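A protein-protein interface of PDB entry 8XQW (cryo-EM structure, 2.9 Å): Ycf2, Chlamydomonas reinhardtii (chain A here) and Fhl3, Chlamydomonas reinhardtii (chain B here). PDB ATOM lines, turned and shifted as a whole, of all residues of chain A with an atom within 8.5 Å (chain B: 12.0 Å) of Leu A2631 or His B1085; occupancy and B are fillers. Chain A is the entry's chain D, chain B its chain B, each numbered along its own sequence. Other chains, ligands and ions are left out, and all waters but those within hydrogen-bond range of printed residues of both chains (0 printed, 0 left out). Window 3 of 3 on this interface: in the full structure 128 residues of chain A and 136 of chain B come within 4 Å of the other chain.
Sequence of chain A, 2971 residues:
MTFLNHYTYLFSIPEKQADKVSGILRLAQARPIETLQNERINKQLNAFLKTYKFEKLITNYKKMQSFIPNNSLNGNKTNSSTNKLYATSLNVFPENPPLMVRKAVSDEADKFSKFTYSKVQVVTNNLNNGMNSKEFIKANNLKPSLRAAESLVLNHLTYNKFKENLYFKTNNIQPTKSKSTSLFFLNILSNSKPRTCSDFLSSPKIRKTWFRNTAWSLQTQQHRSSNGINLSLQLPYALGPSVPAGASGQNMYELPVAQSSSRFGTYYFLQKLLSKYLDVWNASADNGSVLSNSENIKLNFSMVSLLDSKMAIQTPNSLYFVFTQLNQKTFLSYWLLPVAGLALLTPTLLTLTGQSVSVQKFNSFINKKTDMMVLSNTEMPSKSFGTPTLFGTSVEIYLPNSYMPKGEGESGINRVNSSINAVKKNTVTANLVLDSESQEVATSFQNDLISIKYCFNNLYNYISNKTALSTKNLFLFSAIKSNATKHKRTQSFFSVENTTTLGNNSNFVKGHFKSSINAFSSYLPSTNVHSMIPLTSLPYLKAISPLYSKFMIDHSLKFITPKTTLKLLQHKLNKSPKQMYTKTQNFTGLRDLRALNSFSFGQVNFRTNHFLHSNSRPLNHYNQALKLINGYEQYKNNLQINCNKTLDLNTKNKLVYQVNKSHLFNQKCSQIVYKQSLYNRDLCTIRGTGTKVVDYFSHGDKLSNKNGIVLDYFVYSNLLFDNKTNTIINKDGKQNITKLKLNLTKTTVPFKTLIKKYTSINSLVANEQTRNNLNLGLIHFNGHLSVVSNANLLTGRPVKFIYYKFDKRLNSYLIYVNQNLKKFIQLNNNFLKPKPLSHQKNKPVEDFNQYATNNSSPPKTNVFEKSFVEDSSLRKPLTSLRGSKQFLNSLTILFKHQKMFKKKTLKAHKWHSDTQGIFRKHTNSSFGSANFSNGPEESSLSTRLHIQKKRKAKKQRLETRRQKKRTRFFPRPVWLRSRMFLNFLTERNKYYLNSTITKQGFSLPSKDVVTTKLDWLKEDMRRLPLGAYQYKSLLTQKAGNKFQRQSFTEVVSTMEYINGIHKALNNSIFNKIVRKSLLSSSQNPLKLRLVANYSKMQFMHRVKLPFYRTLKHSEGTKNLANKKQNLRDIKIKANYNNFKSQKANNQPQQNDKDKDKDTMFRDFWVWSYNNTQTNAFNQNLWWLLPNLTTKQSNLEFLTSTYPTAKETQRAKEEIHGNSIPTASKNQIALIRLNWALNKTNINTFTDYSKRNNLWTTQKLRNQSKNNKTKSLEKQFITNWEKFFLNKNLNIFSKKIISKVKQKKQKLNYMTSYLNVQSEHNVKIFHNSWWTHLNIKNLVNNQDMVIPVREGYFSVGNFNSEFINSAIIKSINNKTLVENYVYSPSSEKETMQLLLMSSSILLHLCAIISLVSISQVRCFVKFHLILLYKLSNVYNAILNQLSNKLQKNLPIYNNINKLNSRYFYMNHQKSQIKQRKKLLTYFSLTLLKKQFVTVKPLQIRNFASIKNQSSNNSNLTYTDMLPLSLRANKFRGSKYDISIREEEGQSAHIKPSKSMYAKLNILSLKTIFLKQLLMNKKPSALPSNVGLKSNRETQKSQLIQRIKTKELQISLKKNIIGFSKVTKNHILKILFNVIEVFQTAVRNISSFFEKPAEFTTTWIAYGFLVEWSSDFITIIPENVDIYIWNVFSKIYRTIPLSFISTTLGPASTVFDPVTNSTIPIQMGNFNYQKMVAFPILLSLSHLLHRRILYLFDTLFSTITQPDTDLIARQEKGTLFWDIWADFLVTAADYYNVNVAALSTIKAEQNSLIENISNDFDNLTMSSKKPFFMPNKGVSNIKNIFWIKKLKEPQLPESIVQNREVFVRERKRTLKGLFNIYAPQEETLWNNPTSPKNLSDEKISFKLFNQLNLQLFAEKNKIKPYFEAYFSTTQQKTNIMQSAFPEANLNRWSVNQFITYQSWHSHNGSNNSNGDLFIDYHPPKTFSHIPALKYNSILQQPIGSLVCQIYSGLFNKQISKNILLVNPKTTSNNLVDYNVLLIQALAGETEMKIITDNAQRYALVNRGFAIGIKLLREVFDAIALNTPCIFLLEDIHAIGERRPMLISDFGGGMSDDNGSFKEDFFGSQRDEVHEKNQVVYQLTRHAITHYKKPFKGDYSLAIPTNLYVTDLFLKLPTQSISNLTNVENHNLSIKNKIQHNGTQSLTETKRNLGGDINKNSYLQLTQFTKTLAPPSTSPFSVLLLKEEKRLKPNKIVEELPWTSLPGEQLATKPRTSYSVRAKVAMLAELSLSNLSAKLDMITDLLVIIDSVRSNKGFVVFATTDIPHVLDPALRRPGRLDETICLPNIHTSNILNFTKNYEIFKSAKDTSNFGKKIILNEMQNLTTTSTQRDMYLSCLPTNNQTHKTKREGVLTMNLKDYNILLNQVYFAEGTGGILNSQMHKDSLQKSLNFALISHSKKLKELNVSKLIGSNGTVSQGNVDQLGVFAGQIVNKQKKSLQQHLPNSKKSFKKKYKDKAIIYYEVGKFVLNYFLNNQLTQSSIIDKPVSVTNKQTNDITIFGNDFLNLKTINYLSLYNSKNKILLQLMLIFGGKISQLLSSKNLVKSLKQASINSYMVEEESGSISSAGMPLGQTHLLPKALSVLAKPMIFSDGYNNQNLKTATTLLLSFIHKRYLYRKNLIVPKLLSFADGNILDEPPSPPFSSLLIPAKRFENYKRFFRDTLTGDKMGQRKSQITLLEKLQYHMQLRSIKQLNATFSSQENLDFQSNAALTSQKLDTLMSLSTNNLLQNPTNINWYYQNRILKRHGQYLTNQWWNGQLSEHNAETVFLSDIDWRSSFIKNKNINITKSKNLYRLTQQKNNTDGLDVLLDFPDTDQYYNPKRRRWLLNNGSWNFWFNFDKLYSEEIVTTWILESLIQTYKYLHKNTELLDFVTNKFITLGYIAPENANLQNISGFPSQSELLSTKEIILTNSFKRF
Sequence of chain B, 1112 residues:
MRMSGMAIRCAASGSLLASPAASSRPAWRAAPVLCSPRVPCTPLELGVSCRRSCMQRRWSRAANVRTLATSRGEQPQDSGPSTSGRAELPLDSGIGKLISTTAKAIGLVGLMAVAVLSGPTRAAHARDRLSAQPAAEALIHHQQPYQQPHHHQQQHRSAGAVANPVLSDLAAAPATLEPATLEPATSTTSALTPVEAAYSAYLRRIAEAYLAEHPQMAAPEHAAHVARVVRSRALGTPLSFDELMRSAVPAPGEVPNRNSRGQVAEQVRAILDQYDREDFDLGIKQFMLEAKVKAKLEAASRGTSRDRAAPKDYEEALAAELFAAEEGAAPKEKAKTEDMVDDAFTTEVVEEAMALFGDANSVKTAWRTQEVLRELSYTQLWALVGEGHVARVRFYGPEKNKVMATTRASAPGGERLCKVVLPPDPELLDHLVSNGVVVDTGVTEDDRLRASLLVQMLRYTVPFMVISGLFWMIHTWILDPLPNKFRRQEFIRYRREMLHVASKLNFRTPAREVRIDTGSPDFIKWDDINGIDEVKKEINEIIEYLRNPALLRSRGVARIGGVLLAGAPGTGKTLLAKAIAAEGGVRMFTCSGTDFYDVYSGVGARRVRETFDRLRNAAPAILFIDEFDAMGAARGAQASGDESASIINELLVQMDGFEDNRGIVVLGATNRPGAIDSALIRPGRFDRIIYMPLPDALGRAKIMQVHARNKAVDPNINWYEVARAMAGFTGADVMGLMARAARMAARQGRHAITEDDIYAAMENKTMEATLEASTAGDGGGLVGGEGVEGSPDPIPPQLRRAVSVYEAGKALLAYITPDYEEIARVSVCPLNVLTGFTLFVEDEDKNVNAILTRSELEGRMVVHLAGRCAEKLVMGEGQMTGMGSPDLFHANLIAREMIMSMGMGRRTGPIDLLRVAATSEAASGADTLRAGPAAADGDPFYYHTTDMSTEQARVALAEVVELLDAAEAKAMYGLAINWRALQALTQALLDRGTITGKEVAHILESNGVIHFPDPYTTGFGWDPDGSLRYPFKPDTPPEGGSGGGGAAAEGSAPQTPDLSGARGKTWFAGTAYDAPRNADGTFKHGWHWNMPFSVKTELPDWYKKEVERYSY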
ATOM      1  N   PRO A2625      -7.821   8.689  -9.287  1.00  0.00           N
ATOM      2  CA  PRO A2625      -8.412   7.770 -10.265  1.00  0.00           C
ATOM      3  C   PRO A2625      -7.942   6.339 -10.120  1.00  0.00           C
ATOM      4  O   PRO A2625      -8.622   5.427 -10.600  1.00  0.00           O
ATOM      5  CB  PRO A2625      -7.980   8.373 -11.605  1.00  0.00           C
ATOM      6  CG  PRO A2625      -7.812   9.790 -11.322  1.00  0.00           C
ATOM      7  CD  PRO A2625      -7.245   9.869  -9.943  1.00  0.00           C
ATOM      8  N   GLY A2627      -7.947   4.929  -7.334  1.00  0.00           N
ATOM      9  CA  GLY A2627      -8.637   4.429  -6.162  1.00  0.00           C
ATOM     10  C   GLY A2627      -9.936   3.722  -6.460  1.00  0.00           C
ATOM     11  O   GLY A2627     -10.385   2.912  -5.645  1.00  0.00           O
ATOM     12  N   GLN A2628     -10.552   4.012  -7.602  1.00  0.00           N
ATOM     13  CA  GLN A2628     -11.784   3.339  -7.984  1.00  0.00           C
ATOM     14  C   GLN A2628     -11.516   1.866  -8.253  1.00  0.00           C
ATOM     15  O   GLN A2628     -10.627   1.519  -9.035  1.00  0.00           O
ATOM     16  CB  GLN A2628     -12.388   4.002  -9.215  1.00  0.00           C
ATOM     17  CG  GLN A2628     -13.340   5.130  -8.897  1.00  0.00           C
ATOM     18  CD  GLN A2628     -12.628   6.434  -8.634  1.00  0.00           C
ATOM     19  OE1 GLN A2628     -11.713   6.501  -7.817  1.00  0.00           O
ATOM     20  NE2 GLN A2628     -13.043   7.483  -9.329  1.00  0.00           N
ATOM     21  N   THR A2629     -12.286   1.002  -7.603  1.00  0.00           N
ATOM     22  CA  THR A2629     -12.058  -0.437  -7.609  1.00  0.00           C
ATOM     23  C   THR A2629     -13.234  -1.183  -8.228  1.00  0.00           C
ATOM     24  O   THR A2629     -13.487  -2.349  -7.922  1.00  0.00           O
ATOM     25  CB  THR A2629     -11.782  -0.941  -6.197  1.00  0.00           C
ATOM     26  OG1 THR A2629     -11.366  -2.309  -6.248  1.00  0.00           O
ATOM     27  CG2 THR A2629     -13.020  -0.802  -5.313  1.00  0.00           C
ATOM     28  N   HIS A2630     -14.087  -0.423  -8.914  1.00  0.00           N
ATOM     29  CA  HIS A2630     -15.311  -1.019  -9.501  1.00  0.00           C
ATOM     30  C   HIS A2630     -15.283  -0.716 -10.994  1.00  0.00           C
ATOM     31  O   HIS A2630     -14.199  -0.913 -11.566  1.00  0.00           O
ATOM     32  CB  HIS A2630     -16.551  -0.413  -8.849  1.00  0.00           C
ATOM     33  CG  HIS A2630     -16.299   0.944  -8.285  1.00  0.00           C
ATOM     34  ND1 HIS A2630     -16.546   2.095  -9.001  1.00  0.00           N
ATOM     35  CD2 HIS A2630     -15.824   1.342  -7.097  1.00  0.00           C
ATOM     36  CE1 HIS A2630     -16.230   3.146  -8.261  1.00  0.00           C
ATOM     37  NE2 HIS A2630     -15.786   2.711  -7.103  1.00  0.00           N
ATOM     38  N   LEU A2631     -16.397  -0.253 -11.567  1.00  0.00           N
ATOM     39  CA  LEU A2631     -16.451   0.144 -12.999  1.00  0.00           C
ATOM     40  C   LEU A2631     -15.826  -0.925 -13.913  1.00  0.00           C
ATOM     41  O   LEU A2631     -14.600  -0.875 -14.128  1.00  0.00           O
ATOM     42  CB  LEU A2631     -15.732   1.481 -13.128  1.00  0.00           C
ATOM     43  CG  LEU A2631     -16.405   2.684 -12.465  1.00  0.00           C
ATOM     44  CD1 LEU A2631     -15.438   3.855 -12.452  1.00  0.00           C
ATOM     45  CD2 LEU A2631     -17.669   3.040 -13.224  1.00  0.00           C
ATOM     46  N   LEU A2632     -16.643  -1.803 -14.494  1.00  0.00           N
ATOM     47  CA  LEU A2632     -16.148  -2.838 -15.438  1.00  0.00           C
ATOM     48  C   LEU A2632     -14.812  -2.437 -16.072  1.00  0.00           C
ATOM     49  O   LEU A2632     -14.778  -1.425 -16.791  1.00  0.00           O
ATOM     50  CB  LEU A2632     -17.224  -3.011 -16.502  1.00  0.00           C
ATOM     51  CG  LEU A2632     -18.057  -4.293 -16.416  1.00  0.00           C
ATOM     52  CD1 LEU A2632     -17.307  -5.389 -15.683  1.00  0.00           C
ATOM     53  CD2 LEU A2632     -19.390  -4.014 -15.749  1.00  0.00           C
ATOM     54  N   PRO A2633     -13.738  -3.232 -15.913  1.00  0.00           N
ATOM     55  CA  PRO A2633     -12.415  -2.865 -16.418  1.00  0.00           C
ATOM     56  C   PRO A2633     -12.202  -2.140 -17.752  1.00  0.00           C
ATOM     57  O   PRO A2633     -11.055  -1.745 -18.002  1.00  0.00           O
ATOM     58  CB  PRO A2633     -11.800  -4.265 -16.488  1.00  0.00           C
ATOM     59  CG  PRO A2633     -12.313  -4.940 -15.248  1.00  0.00           C
ATOM     60  CD  PRO A2633     -13.760  -4.500 -15.210  1.00  0.00           C
ATOM     61  N   LYS A2634     -13.224  -1.994 -18.590  1.00  0.00           N
ATOM     62  CA  LYS A2634     -13.052  -1.220 -19.843  1.00  0.00           C
ATOM     63  C   LYS A2634     -13.414   0.234 -19.567  1.00  0.00           C
ATOM     64  O   LYS A2634     -12.670   1.138 -19.977  1.00  0.00           O
ATOM     65  CB  LYS A2634     -13.974  -1.701 -20.965  1.00  0.00           C
ATOM     66  CG  LYS A2634     -13.416  -1.532 -22.368  1.00  0.00           C
ATOM     67  CD  LYS A2634     -14.325  -0.720 -23.281  1.00  0.00           C
ATOM     68  CE  LYS A2634     -14.423  -1.313 -24.652  1.00  0.00           C
ATOM     69  NZ  LYS A2634     -15.645  -0.902 -25.351  1.00  0.00           N
ATOM     70  N   ALA A2635     -14.541   0.433 -18.903  1.00  0.00           N
ATOM     71  CA  ALA A2635     -14.903   1.804 -18.575  1.00  0.00           C
ATOM     72  C   ALA A2635     -14.041   2.394 -17.476  1.00  0.00           C
ATOM     73  O   ALA A2635     -14.204   3.571 -17.147  1.00  0.00           O
ATOM     74  CB  ALA A2635     -16.371   1.885 -18.154  1.00  0.00           C
ATOM     75  N   LEU A2636     -13.150   1.602 -16.892  1.00  0.00           N
ATOM     76  CA  LEU A2636     -12.199   2.111 -15.920  1.00  0.00           C
ATOM     77  C   LEU A2636     -10.971   2.712 -16.576  1.00  0.00           C
ATOM     78  O   LEU A2636     -10.337   3.591 -15.991  1.00  0.00           O
ATOM     79  CB  LEU A2636     -11.784   0.988 -14.976  1.00  0.00           C
ATOM     80  CG  LEU A2636     -10.616   1.230 -14.031  1.00  0.00           C
ATOM     81  CD1 LEU A2636     -11.019   2.220 -12.971  1.00  0.00           C
ATOM     82  CD2 LEU A2636     -10.179  -0.071 -13.404  1.00  0.00           C
ATOM     83  N   SER A2637     -10.638   2.281 -17.785  1.00  0.00           N
ATOM     84  CA  SER A2637      -9.427   2.732 -18.448  1.00  0.00           C
ATOM     85  C   SER A2637      -9.539   4.123 -19.056  1.00  0.00           C
ATOM     86  O   SER A2637      -8.618   4.538 -19.764  1.00  0.00           O
ATOM     87  CB  SER A2637      -9.045   1.740 -19.538  1.00  0.00           C
ATOM     88  OG  SER A2637      -9.849   1.943 -20.682  1.00  0.00           O
ATOM     89  N   VAL A2638     -10.628   4.853 -18.817  1.00  0.00           N
ATOM     90  CA  VAL A2638     -10.779   6.198 -19.355  1.00  0.00           C
ATOM     91  C   VAL A2638     -10.756   7.256 -18.266  1.00  0.00           C
ATOM     92  O   VAL A2638     -11.004   8.425 -18.549  1.00  0.00           O
ATOM     93  CB  VAL A2638     -12.057   6.329 -20.188  1.00  0.00           C
ATOM     94  CG1 VAL A2638     -12.072   5.302 -21.274  1.00  0.00           C
ATOM     95  CG2 VAL A2638     -13.254   6.175 -19.308  1.00  0.00           C
ATOM     96  N   LEU A2639     -10.457   6.882 -17.028  1.00  0.00           N
ATOM     97  CA  LEU A2639     -10.508   7.864 -15.954  1.00  0.00           C
ATOM     98  C   LEU A2639      -9.354   8.851 -16.038  1.00  0.00           C
ATOM     99  O   LEU A2639      -9.395   9.910 -15.407  1.00  0.00           O
ATOM    100  CB  LEU A2639     -10.505   7.168 -14.601  1.00  0.00           C
ATOM    101  CG  LEU A2639     -11.700   6.287 -14.291  1.00  0.00           C
ATOM    102  CD1 LEU A2639     -11.702   5.956 -12.826  1.00  0.00           C
ATOM    103  CD2 LEU A2639     -12.973   6.979 -14.682  1.00  0.00           C
ATOM    104  N   HIS B1085     -20.099   4.068 -16.287  1.00  0.00           N
ATOM    105  CA  HIS B1085     -19.805   5.392 -16.814  1.00  0.00           C
ATOM    106  C   HIS B1085     -18.650   6.029 -16.057  1.00  0.00           C
ATOM    107  O   HIS B1085     -17.508   5.599 -16.179  1.00  0.00           O
ATOM    108  CB  HIS B1085     -21.041   6.280 -16.738  1.00  0.00           C
ATOM    109  CG  HIS B1085     -21.242   7.145 -17.942  1.00  0.00           C
ATOM    110  ND1 HIS B1085     -20.518   8.298 -18.159  1.00  0.00           N
ATOM    111  CD2 HIS B1085     -22.091   7.033 -18.989  1.00  0.00           C
ATOM    112  CE1 HIS B1085     -20.915   8.857 -19.286  1.00  0.00           C
ATOM    113  NE2 HIS B1085     -21.870   8.110 -19.809  1.00  0.00           N
ATOM    114  N   GLY B1086     -18.955   7.050 -15.267  1.00  0.00           N
ATOM    115  CA  GLY B1086     -17.920   7.776 -14.561  1.00  0.00           C
ATOM    116  C   GLY B1086     -17.368   8.897 -15.408  1.00  0.00           C
ATOM    117  O   GLY B1086     -17.954   9.243 -16.434  1.00  0.00           O
ATOM    118  N   TRP B1087     -16.242   9.468 -15.006  1.00  0.00           N
ATOM    119  CA  TRP B1087     -15.665  10.546 -15.785  1.00  0.00           C
ATOM    120  C   TRP B1087     -15.021  10.006 -17.054  1.00  0.00           C
ATOM    121  O   TRP B1087     -14.883   8.802 -17.255  1.00  0.00           O
ATOM    122  CB  TRP B1087     -14.629  11.310 -14.973  1.00  0.00           C
ATOM    123  CG  TRP B1087     -15.175  12.145 -13.873  1.00  0.00           C
ATOM    124  CD1 TRP B1087     -14.713  12.201 -12.597  1.00  0.00           C
ATOM    125  CD2 TRP B1087     -16.267  13.069 -13.942  1.00  0.00           C
ATOM    126  NE1 TRP B1087     -15.450  13.094 -11.862  1.00  0.00           N
ATOM    127  CE2 TRP B1087     -16.411  13.641 -12.667  1.00  0.00           C
ATOM    128  CE3 TRP B1087     -17.143  13.463 -14.954  1.00  0.00           C
ATOM    129  CZ2 TRP B1087     -17.388  14.580 -12.382  1.00  0.00           C
ATOM    130  CZ3 TRP B1087     -18.109  14.399 -14.666  1.00  0.00           C
ATOM    131  CH2 TRP B1087     -18.227  14.946 -13.393  1.00  0.00           C
ATOM    132  N   HIS B1088     -14.622  10.930 -17.917  1.00  0.00           N
ATOM    133  CA  HIS B1088     -13.805  10.633 -19.076  1.00  0.00           C
ATOM    134  C   HIS B1088     -12.575  11.520 -19.004  1.00  0.00           C
ATOM    135  O   HIS B1088     -12.638  12.638 -18.504  1.00  0.00           O
ATOM    136  CB  HIS B1088     -14.572  10.859 -20.376  1.00  0.00           C
ATOM    137  CG  HIS B1088     -13.853  10.389 -21.594  1.00  0.00           C
ATOM    138  ND1 HIS B1088     -13.887   9.085 -22.023  1.00  0.00           N
ATOM    139  CD2 HIS B1088     -13.096  11.055 -22.490  1.00  0.00           C
ATOM    140  CE1 HIS B1088     -13.167   8.964 -23.120  1.00  0.00           C
ATOM    141  NE2 HIS B1088     -12.677  10.146 -23.428  1.00  0.00           N
ATOM    142  N   TRP B1089     -11.448  11.017 -19.481  1.00  0.00           N
ATOM    143  CA  TRP B1089     -10.231  11.797 -19.344  1.00  0.00           C
ATOM    144  C   TRP B1089     -10.200  13.008 -20.253  1.00  0.00           C
ATOM    145  O   TRP B1089      -9.229  13.759 -20.203  1.00  0.00           O
ATOM    146  CB  TRP B1089      -9.009  10.930 -19.627  1.00  0.00           C
ATOM    147  CG  TRP B1089      -8.887  10.507 -21.040  1.00  0.00           C
ATOM    148  CD1 TRP B1089      -9.432   9.410 -21.604  1.00  0.00           C
ATOM    149  CD2 TRP B1089      -8.159  11.168 -22.070  1.00  0.00           C
ATOM    150  NE1 TRP B1089      -9.105   9.345 -22.927  1.00  0.00           N
ATOM    151  CE2 TRP B1089      -8.323  10.419 -23.238  1.00  0.00           C
ATOM    152  CE3 TRP B1089      -7.391  12.327 -22.119  1.00  0.00           C
ATOM    153  CZ2 TRP B1089      -7.750  10.785 -24.435  1.00  0.00           C
ATOM    154  CZ3 TRP B1089      -6.827  12.688 -23.309  1.00  0.00           C
ATOM    155  CH2 TRP B1089      -7.006  11.921 -24.449  1.00  0.00           C
ATOM    156  N   ASN B1090     -11.227  13.234 -21.057  1.00  0.00           N
ATOM    157  CA  ASN B1090     -11.201  14.205 -22.137  1.00  0.00           C
ATOM    158  C   ASN B1090     -12.454  15.049 -22.121  1.00  0.00           C
ATOM    159  O   ASN B1090     -13.082  15.288 -23.148  1.00  0.00           O
ATOM    160  CB  ASN B1090     -11.070  13.487 -23.467  1.00  0.00           C
ATOM    161  CG  ASN B1090     -10.415  14.318 -24.513  1.00  0.00           C
ATOM    162  OD1 ASN B1090      -9.782  15.315 -24.209  1.00  0.00           O
ATOM    163  ND2 ASN B1090     -10.552  13.913 -25.758  1.00  0.00           N
ATOM    164  N   MET B1091     -12.833  15.507 -20.971  1.00  0.00           N
ATOM    165  CA  MET B1091     -14.060  16.277 -20.881  1.00  0.00           C
ATOM    166  C   MET B1091     -13.814  17.720 -21.299  1.00  0.00           C
ATOM    167  O   MET B1091     -12.746  18.264 -21.034  1.00  0.00           O
ATOM    168  CB  MET B1091     -14.595  16.261 -19.471  1.00  0.00           C
ATOM    169  CG  MET B1091     -14.568  14.927 -18.839  1.00  0.00           C
ATOM    170  SD  MET B1091     -15.947  14.782 -17.732  1.00  0.00           S
ATOM    171  CE  MET B1091     -17.197  15.546 -18.736  1.00  0.00           C
ATOM    172  N   PRO B1092     -14.784  18.359 -21.937  1.00  0.00           N
ATOM    173  CA  PRO B1092     -14.645  19.778 -22.245  1.00  0.00           C
ATOM    174  C   PRO B1092     -14.614  20.605 -20.974  1.00  0.00           C
ATOM    175  O   PRO B1092     -15.109  20.190 -19.928  1.00  0.00           O
ATOM    176  CB  PRO B1092     -15.893  20.079 -23.073  1.00  0.00           C
ATOM    177  CG  PRO B1092     -16.357  18.774 -23.536  1.00  0.00           C
ATOM    178  CD  PRO B1092     -16.034  17.816 -22.470  1.00  0.00           C
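Of the 8 printed residues of chain B, 4 touch a printed residue of chain A.
Hydrophobic or aromatic side chains of chain B within 4 Å of the printed part of chain A: His B1088 and Trp B1089.
Hydrophobic or aromatic side chains of chain A within 4 Å of the printed part of chain B: Leu A2631, Val A2638 and Leu A2639.
Among the printed residues, no Asp or Glu carboxylate lies within 4 Å of a Lys or Arg side-chain nitrogen of the other chain.
No residue of chain B comes within 4 Å of Gln A2628.
Of chain B, only His B1085 comes within 4 Å of Leu A2631.
No residue of chain B comes within 4 Å of Leu A2632.
No residue of chain B comes within 4 Å of Pro A2633.
No residue of chain B comes within 4 Å of Leu A2636.
Of chain B, only Trp B1087, His B1088 and Trp B1089 come within 4 Å of Val A2638.
Printed residues of chain B within 4 Å of Leu A2639: Trp B1087.
Printed residues of chain A within 4 Å of His B1085: Leu A2631 and Ala A2635.
Of the printed residues of chain A, His B1088 touches Val A2638 (3.5 Å).
Of the printed residues of chain A, Trp B1089 touches Val A2638.
Asn B1090 touches none of the printed residues of chain A.
Pro B1092 touches none of the printed residues of chain A.
The nearest printed residue of chain A that does not touch His B1085 is Leu A2639 (5.0 Å).
The nearest printed residue of chain A that does not touch Trp B1089 is Leu A2639 (4.2 Å).
Among the printed residues, pairs that only touch across the chains: Leu A2631 with His B1085 (3.9 Å), Ala A2635 with His B1085 (3.996 Å), Val A2638 with Trp B1087 (3.7 Å), Val A2638 with His B1088 (3.5 Å) and Leu A2639 with Trp B1087 (3.7 Å).
N of Trp B1089 sits at hydrogen-bond distance from O of Val A2638 (2.8 Å).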
